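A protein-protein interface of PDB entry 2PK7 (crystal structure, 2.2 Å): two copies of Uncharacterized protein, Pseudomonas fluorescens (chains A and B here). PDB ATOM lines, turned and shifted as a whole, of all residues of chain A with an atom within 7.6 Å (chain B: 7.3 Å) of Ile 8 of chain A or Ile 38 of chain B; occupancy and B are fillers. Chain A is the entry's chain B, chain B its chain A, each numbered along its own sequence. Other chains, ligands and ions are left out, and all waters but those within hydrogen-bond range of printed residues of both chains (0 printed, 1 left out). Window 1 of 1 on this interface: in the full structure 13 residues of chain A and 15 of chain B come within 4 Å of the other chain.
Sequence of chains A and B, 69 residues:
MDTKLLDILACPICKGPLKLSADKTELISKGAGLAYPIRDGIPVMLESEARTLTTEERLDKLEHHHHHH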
ATOM      1  N   THR A   3      27.723  -9.894 -24.823  1.00  0.00           N
ATOM      2  CA  THR A   3      28.147  -9.827 -23.391  1.00  0.00           C
ATOM      3  C   THR A   3      28.539 -11.216 -22.902  1.00  0.00           C
ATOM      4  O   THR A   3      27.770 -12.166 -23.044  1.00  0.00           O
ATOM      5  CB  THR A   3      27.009  -9.270 -22.541  1.00  0.00           C
ATOM      6  N   LYS A   4      29.736 -11.340 -22.337  1.00  0.00           N
ATOM      7  CA  LYS A   4      30.191 -12.630 -21.832  1.00  0.00           C
ATOM      8  C   LYS A   4      30.321 -12.593 -20.312  1.00  0.00           C
ATOM      9  O   LYS A   4      30.527 -11.532 -19.718  1.00  0.00           O
ATOM     10  CB  LYS A   4      31.518 -13.025 -22.487  1.00  0.00           C
ATOM     11  CG  LYS A   4      32.392 -11.853 -22.914  1.00  0.00           C
ATOM     12  CD  LYS A   4      33.667 -12.332 -23.590  1.00  0.00           C
ATOM     13  CE  LYS A   4      34.682 -11.202 -23.712  1.00  0.00           C
ATOM     14  NZ  LYS A   4      34.854 -10.706 -25.105  1.00  0.00           N
ATOM     15  N   LEU A   5      30.194 -13.749 -19.676  1.00  0.00           N
ATOM     16  CA  LEU A   5      30.270 -13.787 -18.227  1.00  0.00           C
ATOM     17  C   LEU A   5      31.486 -13.065 -17.653  1.00  0.00           C
ATOM     18  O   LEU A   5      31.342 -12.203 -16.783  1.00  0.00           O
ATOM     19  CB  LEU A   5      30.242 -15.231 -17.725  1.00  0.00           C
ATOM     20  CG  LEU A   5      30.145 -15.321 -16.196  1.00  0.00           C
ATOM     21  CD1 LEU A   5      28.960 -14.520 -15.706  1.00  0.00           C
ATOM     22  CD2 LEU A   5      30.008 -16.773 -15.778  1.00  0.00           C
ATOM     23  N   LEU A   6      32.676 -13.398 -18.148  1.00  0.00           N
ATOM     24  CA  LEU A   6      33.900 -12.778 -17.652  1.00  0.00           C
ATOM     25  C   LEU A   6      33.871 -11.247 -17.595  1.00  0.00           C
ATOM     26  O   LEU A   6      34.631 -10.650 -16.834  1.00  0.00           O
ATOM     27  CB  LEU A   6      35.114 -13.235 -18.479  1.00  0.00           C
ATOM     28  CG  LEU A   6      36.106 -14.184 -17.791  1.00  0.00           C
ATOM     29  CD1 LEU A   6      37.432 -14.195 -18.549  1.00  0.00           C
ATOM     30  CD2 LEU A   6      36.345 -13.714 -16.360  1.00  0.00           C
ATOM     31  N   ASP A   7      32.996 -10.618 -18.381  1.00  0.00           N
ATOM     32  CA  ASP A   7      32.891  -9.152 -18.406  1.00  0.00           C
ATOM     33  C   ASP A   7      32.068  -8.535 -17.280  1.00  0.00           C
ATOM     34  O   ASP A   7      32.178  -7.342 -17.012  1.00  0.00           O
ATOM     35  CB  ASP A   7      32.288  -8.648 -19.727  1.00  0.00           C
ATOM     36  CG  ASP A   7      33.126  -9.001 -20.933  1.00  0.00           C
ATOM     37  OD1 ASP A   7      34.359  -9.161 -20.793  1.00  0.00           O
ATOM     38  OD2 ASP A   7      32.544  -9.100 -22.033  1.00  0.00           O
ATOM     39  N   ILE A   8      31.226  -9.321 -16.627  1.00  0.00           N
ATOM     40  CA  ILE A   8      30.423  -8.746 -15.557  1.00  0.00           C
ATOM     41  C   ILE A   8      30.843  -9.193 -14.170  1.00  0.00           C
ATOM     42  O   ILE A   8      30.465  -8.579 -13.173  1.00  0.00           O
ATOM     43  CB  ILE A   8      28.941  -9.022 -15.766  1.00  0.00           C
ATOM     44  CG1 ILE A   8      28.693 -10.524 -15.862  1.00  0.00           C
ATOM     45  CG2 ILE A   8      28.466  -8.311 -17.027  1.00  0.00           C
ATOM     46  CD1 ILE A   8      27.250 -10.857 -16.110  1.00  0.00           C
ATOM     47  N   LEU A   9      31.618 -10.266 -14.096  1.00  0.00           N
ATOM     48  CA  LEU A   9      32.100 -10.707 -12.799  1.00  0.00           C
ATOM     49  C   LEU A   9      33.190  -9.693 -12.448  1.00  0.00           C
ATOM     50  O   LEU A   9      33.734  -9.025 -13.330  1.00  0.00           O
ATOM     51  CB  LEU A   9      32.680 -12.126 -12.873  1.00  0.00           C
ATOM     52  CG  LEU A   9      31.690 -13.218 -13.316  1.00  0.00           C
ATOM     53  CD1 LEU A   9      32.291 -14.596 -13.091  1.00  0.00           C
ATOM     54  CD2 LEU A   9      30.404 -13.089 -12.522  1.00  0.00           C
ATOM     55  N   ALA A  10      33.482  -9.547 -11.165  1.00  0.00           N
ATOM     56  CA  ALA A  10      34.506  -8.611 -10.732  1.00  0.00           C
ATOM     57  C   ALA A  10      35.129  -9.178  -9.477  1.00  0.00           C
ATOM     58  O   ALA A  10      34.547 -10.053  -8.830  1.00  0.00           O
ATOM     59  CB  ALA A  10      33.888  -7.237 -10.445  1.00  0.00           C
ATOM     60  N   CYS A  11      36.310  -8.679  -9.134  1.00  0.00           N
ATOM     61  CA  CYS A  11      37.009  -9.151  -7.953  1.00  0.00           C
ATOM     62  C   CYS A  11      36.249  -8.801  -6.680  1.00  0.00           C
ATOM     63  O   CYS A  11      35.822  -7.663  -6.499  1.00  0.00           O
ATOM     64  CB  CYS A  11      38.406  -8.538  -7.888  1.00  0.00           C
ATOM     65  SG  CYS A  11      39.329  -9.021  -6.424  1.00  0.00           S
ATOM     66  N   LEU A  18      38.583  -9.728 -13.978  1.00  0.00           N
ATOM     67  CA  LEU A  18      39.130 -11.065 -13.742  1.00  0.00           C
ATOM     68  C   LEU A  18      39.470 -11.676 -15.085  1.00  0.00           C
ATOM     69  O   LEU A  18      38.817 -11.385 -16.080  1.00  0.00           O
ATOM     70  CB  LEU A  18      38.093 -11.950 -13.055  1.00  0.00           C
ATOM     71  CG  LEU A  18      37.685 -11.493 -11.654  1.00  0.00           C
ATOM     72  CD1 LEU A  18      36.476 -12.277 -11.154  1.00  0.00           C
ATOM     73  CD2 LEU A  18      38.876 -11.683 -10.736  1.00  0.00           C
ATOM     74  N   LYS B  19      23.322 -20.880 -18.412  1.00  0.00           N
ATOM     75  CA  LYS B  19      23.204 -19.882 -19.461  1.00  0.00           C
ATOM     76  C   LYS B  19      23.062 -18.512 -18.830  1.00  0.00           C
ATOM     77  O   LYS B  19      22.381 -18.347 -17.824  1.00  0.00           O
ATOM     78  CB  LYS B  19      21.977 -20.148 -20.352  1.00  0.00           C
ATOM     79  CG  LYS B  19      22.050 -21.424 -21.175  1.00  0.00           C
ATOM     80  CD  LYS B  19      20.884 -21.543 -22.166  1.00  0.00           C
ATOM     81  CE  LYS B  19      19.539 -21.785 -21.488  1.00  0.00           C
ATOM     82  NZ  LYS B  19      19.068 -20.606 -20.713  1.00  0.00           N
ATOM     83  N   LEU B  20      23.723 -17.523 -19.406  1.00  0.00           N
ATOM     84  CA  LEU B  20      23.597 -16.176 -18.880  1.00  0.00           C
ATOM     85  C   LEU B  20      22.176 -15.740 -19.243  1.00  0.00           C
ATOM     86  O   LEU B  20      21.755 -15.912 -20.382  1.00  0.00           O
ATOM     87  CB  LEU B  20      24.645 -15.274 -19.532  1.00  0.00           C
ATOM     88  CG  LEU B  20      24.865 -13.849 -19.016  1.00  0.00           C
ATOM     89  CD1 LEU B  20      24.951 -13.831 -17.496  1.00  0.00           C
ATOM     90  CD2 LEU B  20      26.145 -13.298 -19.636  1.00  0.00           C
ATOM     91  N   SER B  21      21.434 -15.207 -18.273  1.00  0.00           N
ATOM     92  CA  SER B  21      20.063 -14.773 -18.518  1.00  0.00           C
ATOM     93  C   SER B  21      20.029 -13.605 -19.495  1.00  0.00           C
ATOM     94  O   SER B  21      21.052 -12.977 -19.752  1.00  0.00           O
ATOM     95  CB  SER B  21      19.401 -14.343 -17.215  1.00  0.00           C
ATOM     96  OG  SER B  21      20.068 -13.214 -16.674  1.00  0.00           O
ATOM     97  N   ASP B  23      18.735 -10.495 -19.221  1.00  0.00           N
ATOM     98  CA  ASP B  23      19.178  -9.226 -18.635  1.00  0.00           C
ATOM     99  C   ASP B  23      20.581  -9.327 -18.026  1.00  0.00           C
ATOM    100  O   ASP B  23      21.065  -8.385 -17.397  1.00  0.00           O
ATOM    101  CB  ASP B  23      18.181  -8.734 -17.572  1.00  0.00           C
ATOM    102  CG  ASP B  23      18.031  -9.699 -16.409  1.00  0.00           C
ATOM    103  OD1 ASP B  23      18.864 -10.621 -16.282  1.00  0.00           O
ATOM    104  OD2 ASP B  23      17.080  -9.523 -15.611  1.00  0.00           O
ATOM    105  N   LYS B  24      21.223 -10.478 -18.229  1.00  0.00           N
ATOM    106  CA  LYS B  24      22.581 -10.762 -17.744  1.00  0.00           C
ATOM    107  C   LYS B  24      22.804 -10.713 -16.236  1.00  0.00           C
ATOM    108  O   LYS B  24      23.942 -10.593 -15.777  1.00  0.00           O
ATOM    109  CB  LYS B  24      23.603  -9.824 -18.398  1.00  0.00           C
ATOM    110  CG  LYS B  24      23.933 -10.131 -19.852  1.00  0.00           C
ATOM    111  CD  LYS B  24      22.902  -9.560 -20.805  1.00  0.00           C
ATOM    112  CE  LYS B  24      23.311  -9.790 -22.255  1.00  0.00           C
ATOM    113  NZ  LYS B  24      23.534 -11.229 -22.559  1.00  0.00           N
ATOM    114  N   THR B  25      21.741 -10.829 -15.452  1.00  0.00           N
ATOM    115  CA  THR B  25      21.896 -10.764 -14.007  1.00  0.00           C
ATOM    116  C   THR B  25      21.804 -12.120 -13.325  1.00  0.00           C
ATOM    117  O   THR B  25      21.843 -12.210 -12.093  1.00  0.00           O
ATOM    118  CB  THR B  25      20.832  -9.861 -13.389  1.00  0.00           C
ATOM    119  OG1 THR B  25      19.551 -10.497 -13.494  1.00  0.00           O
ATOM    120  CG2 THR B  25      20.788  -8.533 -14.128  1.00  0.00           C
ATOM    121  N   GLU B  26      21.679 -13.183 -14.107  1.00  0.00           N
ATOM    122  CA  GLU B  26      21.564 -14.502 -13.499  1.00  0.00           C
ATOM    123  C   GLU B  26      22.182 -15.573 -14.360  1.00  0.00           C
ATOM    124  O   GLU B  26      22.328 -15.404 -15.561  1.00  0.00           O
ATOM    125  CB  GLU B  26      20.081 -14.877 -13.297  1.00  0.00           C
ATOM    126  CG  GLU B  26      19.276 -13.920 -12.448  1.00  0.00           C
ATOM    127  CD  GLU B  26      17.790 -14.262 -12.467  1.00  0.00           C
ATOM    128  OE1 GLU B  26      17.196 -14.292 -13.567  1.00  0.00           O
ATOM    129  OE2 GLU B  26      17.213 -14.505 -11.384  1.00  0.00           O
ATOM    130  N   LEU B  27      22.539 -16.681 -13.722  1.00  0.00           N
ATOM    131  CA  LEU B  27      23.057 -17.835 -14.419  1.00  0.00           C
ATOM    132  C   LEU B  27      21.926 -18.826 -14.227  1.00  0.00           C
ATOM    133  O   LEU B  27      21.682 -19.310 -13.123  1.00  0.00           O
ATOM    134  CB  LEU B  27      24.347 -18.360 -13.785  1.00  0.00           C
ATOM    135  CG  LEU B  27      25.561 -17.427 -13.883  1.00  0.00           C
ATOM    136  CD1 LEU B  27      26.746 -18.103 -13.230  1.00  0.00           C
ATOM    137  CD2 LEU B  27      25.861 -17.111 -15.333  1.00  0.00           C
ATOM    138  N   ALA B  35      17.720 -20.183 -11.059  1.00  0.00           N
ATOM    139  CA  ALA B  35      18.520 -19.109 -11.649  1.00  0.00           C
ATOM    140  C   ALA B  35      19.371 -18.577 -10.508  1.00  0.00           C
ATOM    141  O   ALA B  35      18.845 -18.160  -9.484  1.00  0.00           O
ATOM    142  CB  ALA B  35      17.631 -17.982 -12.219  1.00  0.00           C
ATOM    143  N   TYR B  36      20.686 -18.611 -10.673  1.00  0.00           N
ATOM    144  CA  TYR B  36      21.573 -18.110  -9.637  1.00  0.00           C
ATOM    145  C   TYR B  36      21.847 -16.632  -9.923  1.00  0.00           C
ATOM    146  O   TYR B  36      22.237 -16.268 -11.032  1.00  0.00           O
ATOM    147  CB  TYR B  36      22.878 -18.910  -9.639  1.00  0.00           C
ATOM    148  CG  TYR B  36      22.676 -20.395  -9.449  1.00  0.00           C
ATOM    149  CD1 TYR B  36      22.240 -20.910  -8.225  1.00  0.00           C
ATOM    150  CD2 TYR B  36      22.901 -21.287 -10.499  1.00  0.00           C
ATOM    151  CE1 TYR B  36      22.045 -22.297  -8.050  1.00  0.00           C
ATOM    152  CE2 TYR B  36      22.708 -22.665 -10.342  1.00  0.00           C
ATOM    153  CZ  TYR B  36      22.281 -23.163  -9.116  1.00  0.00           C
ATOM    154  OH  TYR B  36      22.103 -24.522  -8.966  1.00  0.00           O
ATOM    155  N   PRO B  37      21.638 -15.757  -8.922  1.00  0.00           N
ATOM    156  CA  PRO B  37      21.866 -14.325  -9.096  1.00  0.00           C
ATOM    157  C   PRO B  37      23.335 -13.942  -9.146  1.00  0.00           C
ATOM    158  O   PRO B  37      24.192 -14.590  -8.548  1.00  0.00           O
ATOM    159  CB  PRO B  37      21.169 -13.721  -7.880  1.00  0.00           C
ATOM    160  CG  PRO B  37      21.466 -14.764  -6.807  1.00  0.00           C
ATOM    161  CD  PRO B  37      21.155 -16.048  -7.556  1.00  0.00           C
ATOM    162  N   ILE B  38      23.619 -12.891  -9.893  1.00  0.00           N
ATOM    163  CA  ILE B  38      24.971 -12.378  -9.989  1.00  0.00           C
ATOM    164  C   ILE B  38      24.846 -11.087  -9.219  1.00  0.00           C
ATOM    165  O   ILE B  38      24.112 -10.183  -9.614  1.00  0.00           O
ATOM    166  CB  ILE B  38      25.358 -12.134 -11.445  1.00  0.00           C
ATOM    167  CG1 ILE B  38      25.399 -13.478 -12.177  1.00  0.00           C
ATOM    168  CG2 ILE B  38      26.697 -11.412 -11.525  1.00  0.00           C
ATOM    169  CD1 ILE B  38      25.626 -13.378 -13.665  1.00  0.00           C
ATOM    170  N   ARG B  39      25.539 -11.022  -8.090  1.00  0.00           N
ATOM    171  CA  ARG B  39      25.469  -9.851  -7.231  1.00  0.00           C
ATOM    172  C   ARG B  39      26.786  -9.104  -7.107  1.00  0.00           C
ATOM    173  O   ARG B  39      27.755  -9.622  -6.551  1.00  0.00           O
ATOM    174  CB  ARG B  39      24.978 -10.293  -5.856  1.00  0.00           C
ATOM    175  CG  ARG B  39      23.553 -10.826  -5.891  1.00  0.00           C
ATOM    176  CD  ARG B  39      23.189 -11.551  -4.618  1.00  0.00           C
ATOM    177  NE  ARG B  39      21.768 -11.874  -4.586  1.00  0.00           N
ATOM    178  CZ  ARG B  39      21.208 -12.691  -3.700  1.00  0.00           C
ATOM    179  NH1 ARG B  39      21.953 -13.274  -2.769  1.00  0.00           N
ATOM    180  NH2 ARG B  39      19.906 -12.941  -3.760  1.00  0.00           N
ATOM    181  N   ASP B  40      26.809  -7.878  -7.616  1.00  0.00           N
ATOM    182  CA  ASP B  40      28.008  -7.051  -7.573  1.00  0.00           C
ATOM    183  C   ASP B  40      29.206  -7.842  -8.093  1.00  0.00           C
ATOM    184  O   ASP B  40      30.242  -7.945  -7.439  1.00  0.00           O
ATOM    185  CB  ASP B  40      28.255  -6.564  -6.145  1.00  0.00           C
ATOM    186  CG  ASP B  40      29.155  -5.349  -6.095  1.00  0.00           C
ATOM    187  OD1 ASP B  40      29.317  -4.684  -7.141  1.00  0.00           O
ATOM    188  OD2 ASP B  40      29.686  -5.049  -5.006  1.00  0.00           O
ATOM    189  N   GLY B  41      29.033  -8.414  -9.280  1.00  0.00           N
ATOM    190  CA  GLY B  41      30.087  -9.183  -9.918  1.00  0.00           C
ATOM    191  C   GLY B  41      30.361 -10.576  -9.381  1.00  0.00           C
ATOM    192  O   GLY B  41      31.328 -11.211  -9.797  1.00  0.00           O
ATOM    193  N   ILE B  42      29.523 -11.070  -8.477  1.00  0.00           N
ATOM    194  CA  ILE B  42      29.732 -12.409  -7.928  1.00  0.00           C
ATOM    195  C   ILE B  42      28.536 -13.312  -8.205  1.00  0.00           C
ATOM    196  O   ILE B  42      27.408 -12.972  -7.858  1.00  0.00           O
ATOM    197  CB  ILE B  42      29.968 -12.354  -6.397  1.00  0.00           C
ATOM    198  CG1 ILE B  42      31.157 -11.440  -6.075  1.00  0.00           C
ATOM    199  CG2 ILE B  42      30.228 -13.758  -5.859  1.00  0.00           C
ATOM    200  CD1 ILE B  42      32.467 -11.917  -6.650  1.00  0.00           C
ATOM    201  N   PRO B  43      28.759 -14.470  -8.854  1.00  0.00           N
ATOM    202  CA  PRO B  43      27.635 -15.368  -9.126  1.00  0.00           C
ATOM    203  C   PRO B  43      27.358 -16.181  -7.860  1.00  0.00           C
ATOM    204  O   PRO B  43      28.108 -17.098  -7.538  1.00  0.00           O
ATOM    205  CB  PRO B  43      28.156 -16.228 -10.278  1.00  0.00           C
ATOM    206  CG  PRO B  43      29.618 -16.338  -9.968  1.00  0.00           C
ATOM    207  CD  PRO B  43      29.988 -14.937  -9.519  1.00  0.00           C
ATOM    208  N   VAL B  44      26.299 -15.839  -7.128  1.00  0.00           N
ATOM    209  CA  VAL B  44      25.978 -16.562  -5.898  1.00  0.00           C
ATOM    210  C   VAL B  44      25.205 -17.817  -6.258  1.00  0.00           C
ATOM    211  O   VAL B  44      23.981 -17.807  -6.421  1.00  0.00           O
ATOM    212  CB  VAL B  44      25.160 -15.694  -4.922  1.00  0.00           C
ATOM    213  CG1 VAL B  44      24.896 -16.473  -3.634  1.00  0.00           C
ATOM    214  CG2 VAL B  44      25.924 -14.413  -4.609  1.00  0.00           C
ATOM    215  N   MET B  45      25.942 -18.911  -6.364  1.00  0.00           N
ATOM    216  CA  MET B  45      25.342 -20.167  -6.750  1.00  0.00           C
ATOM    217  C   MET B  45      25.007 -21.174  -5.658  1.00  0.00           C
ATOM    218  O   MET B  45      25.605 -22.249  -5.531  1.00  0.00           O
ATOM    219  CB  MET B  45      26.212 -20.776  -7.825  1.00  0.00           C
ATOM    220  CG  MET B  45      26.218 -19.870  -9.043  1.00  0.00           C
ATOM    221  SD  MET B  45      27.452 -20.471 -10.306  1.00  0.00           S
ATOM    222  CE  MET B  45      26.355 -21.875 -11.005  1.00  0.00           C
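OG of Ser 21 of chain B is in hydrogen-bond range of N of Lys 24 of chain B. The backbone carbonyl oxygen (O) of Thr 25 of chain B lies within hydrogen-bond range of the backbone NH (N) of Ile 38 of chain B (2.9 Å).
Printed residues of chain B within 4 Å of Thr 3 of chain A: Leu 20 and Lys 24. Leu 5 of chain A touches none of the printed residues of chain B. Of the printed residues of chain B, Ile 8 of chain A touches Lys 24 (3.3 Å), Ile 38 (3.9 Å) and Gly 41 (3.3 Å). Of the printed residues of chain B, Leu 9 of chain A touches Gly 41 (3.1 Å) and Pro 43 (3.6 Å). Of the printed residues of chain A, Lys 24 of chain B touches Thr 3 (3.7 Å) and Ile 8 (3.3 Å). Of chain A, only Ile 8 (3.9 Å) comes within 4 Å of Ile 38 of chain B. Printed residues of chain A within 4 Å of Ile 42 of chain B: Ala 10 (3.5 Å). Of the printed residues of chain A, Pro 43 of chain B touches Leu 9. The nearest printed residue of chain B that does not touch Leu 9 of chain A is Ile 38 of chain B (4.2 Å).
No position is printed for both chains. Of the 9 pairs that touch across the chains among the printed residues, none has its exchanged pair printed and touching as well.
The backbone NH (N) of Ala 10 of chain A is in hydrogen-bond range of the backbone carbonyl oxygen (O) of Gly 41 of chain B, 3.0 Å away.
Among the printed residues, merely in contact across the chains: Thr 3 of chain A with Leu 20 of chain B (3.9 Å), Thr 3 of chain A with Lys 24 of chain B (3.7 Å), Ile 8 of chain A with Lys 24 of chain B (3.3 Å), Ile 8 of chain A with Ile 38 of chain B (3.9 Å), Ile 8 of chain A with Gly 41 of chain B (3.3 Å), Leu 9 of chain A with Gly 41 of chain B (3.1 Å), Leu 9 of chain A with Pro 43 of chain B (3.6 Å) and Ala 10 of chain A with Ile 42 of chain B (3.5 Å).
Of the 19 printed residues of chain B, 6 touch a printed residue of chain A. Printed residues of chain B that touch a printed residue of chain A: Leu 20, Lys 24, Ile 38, Gly 41, Ile 42 and Pro 43. Of the 10 printed residues of chain A, 4 touch a printed residue of chain B. Hydrophobic or aromatic side chains of chain A that line the printed part of chain B: Ile 8 and Leu 9. Among the printed residues, no Asp or Glu carboxylate lies within 4 Å of a Lys or Arg side-chain nitrogen of the other chain.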
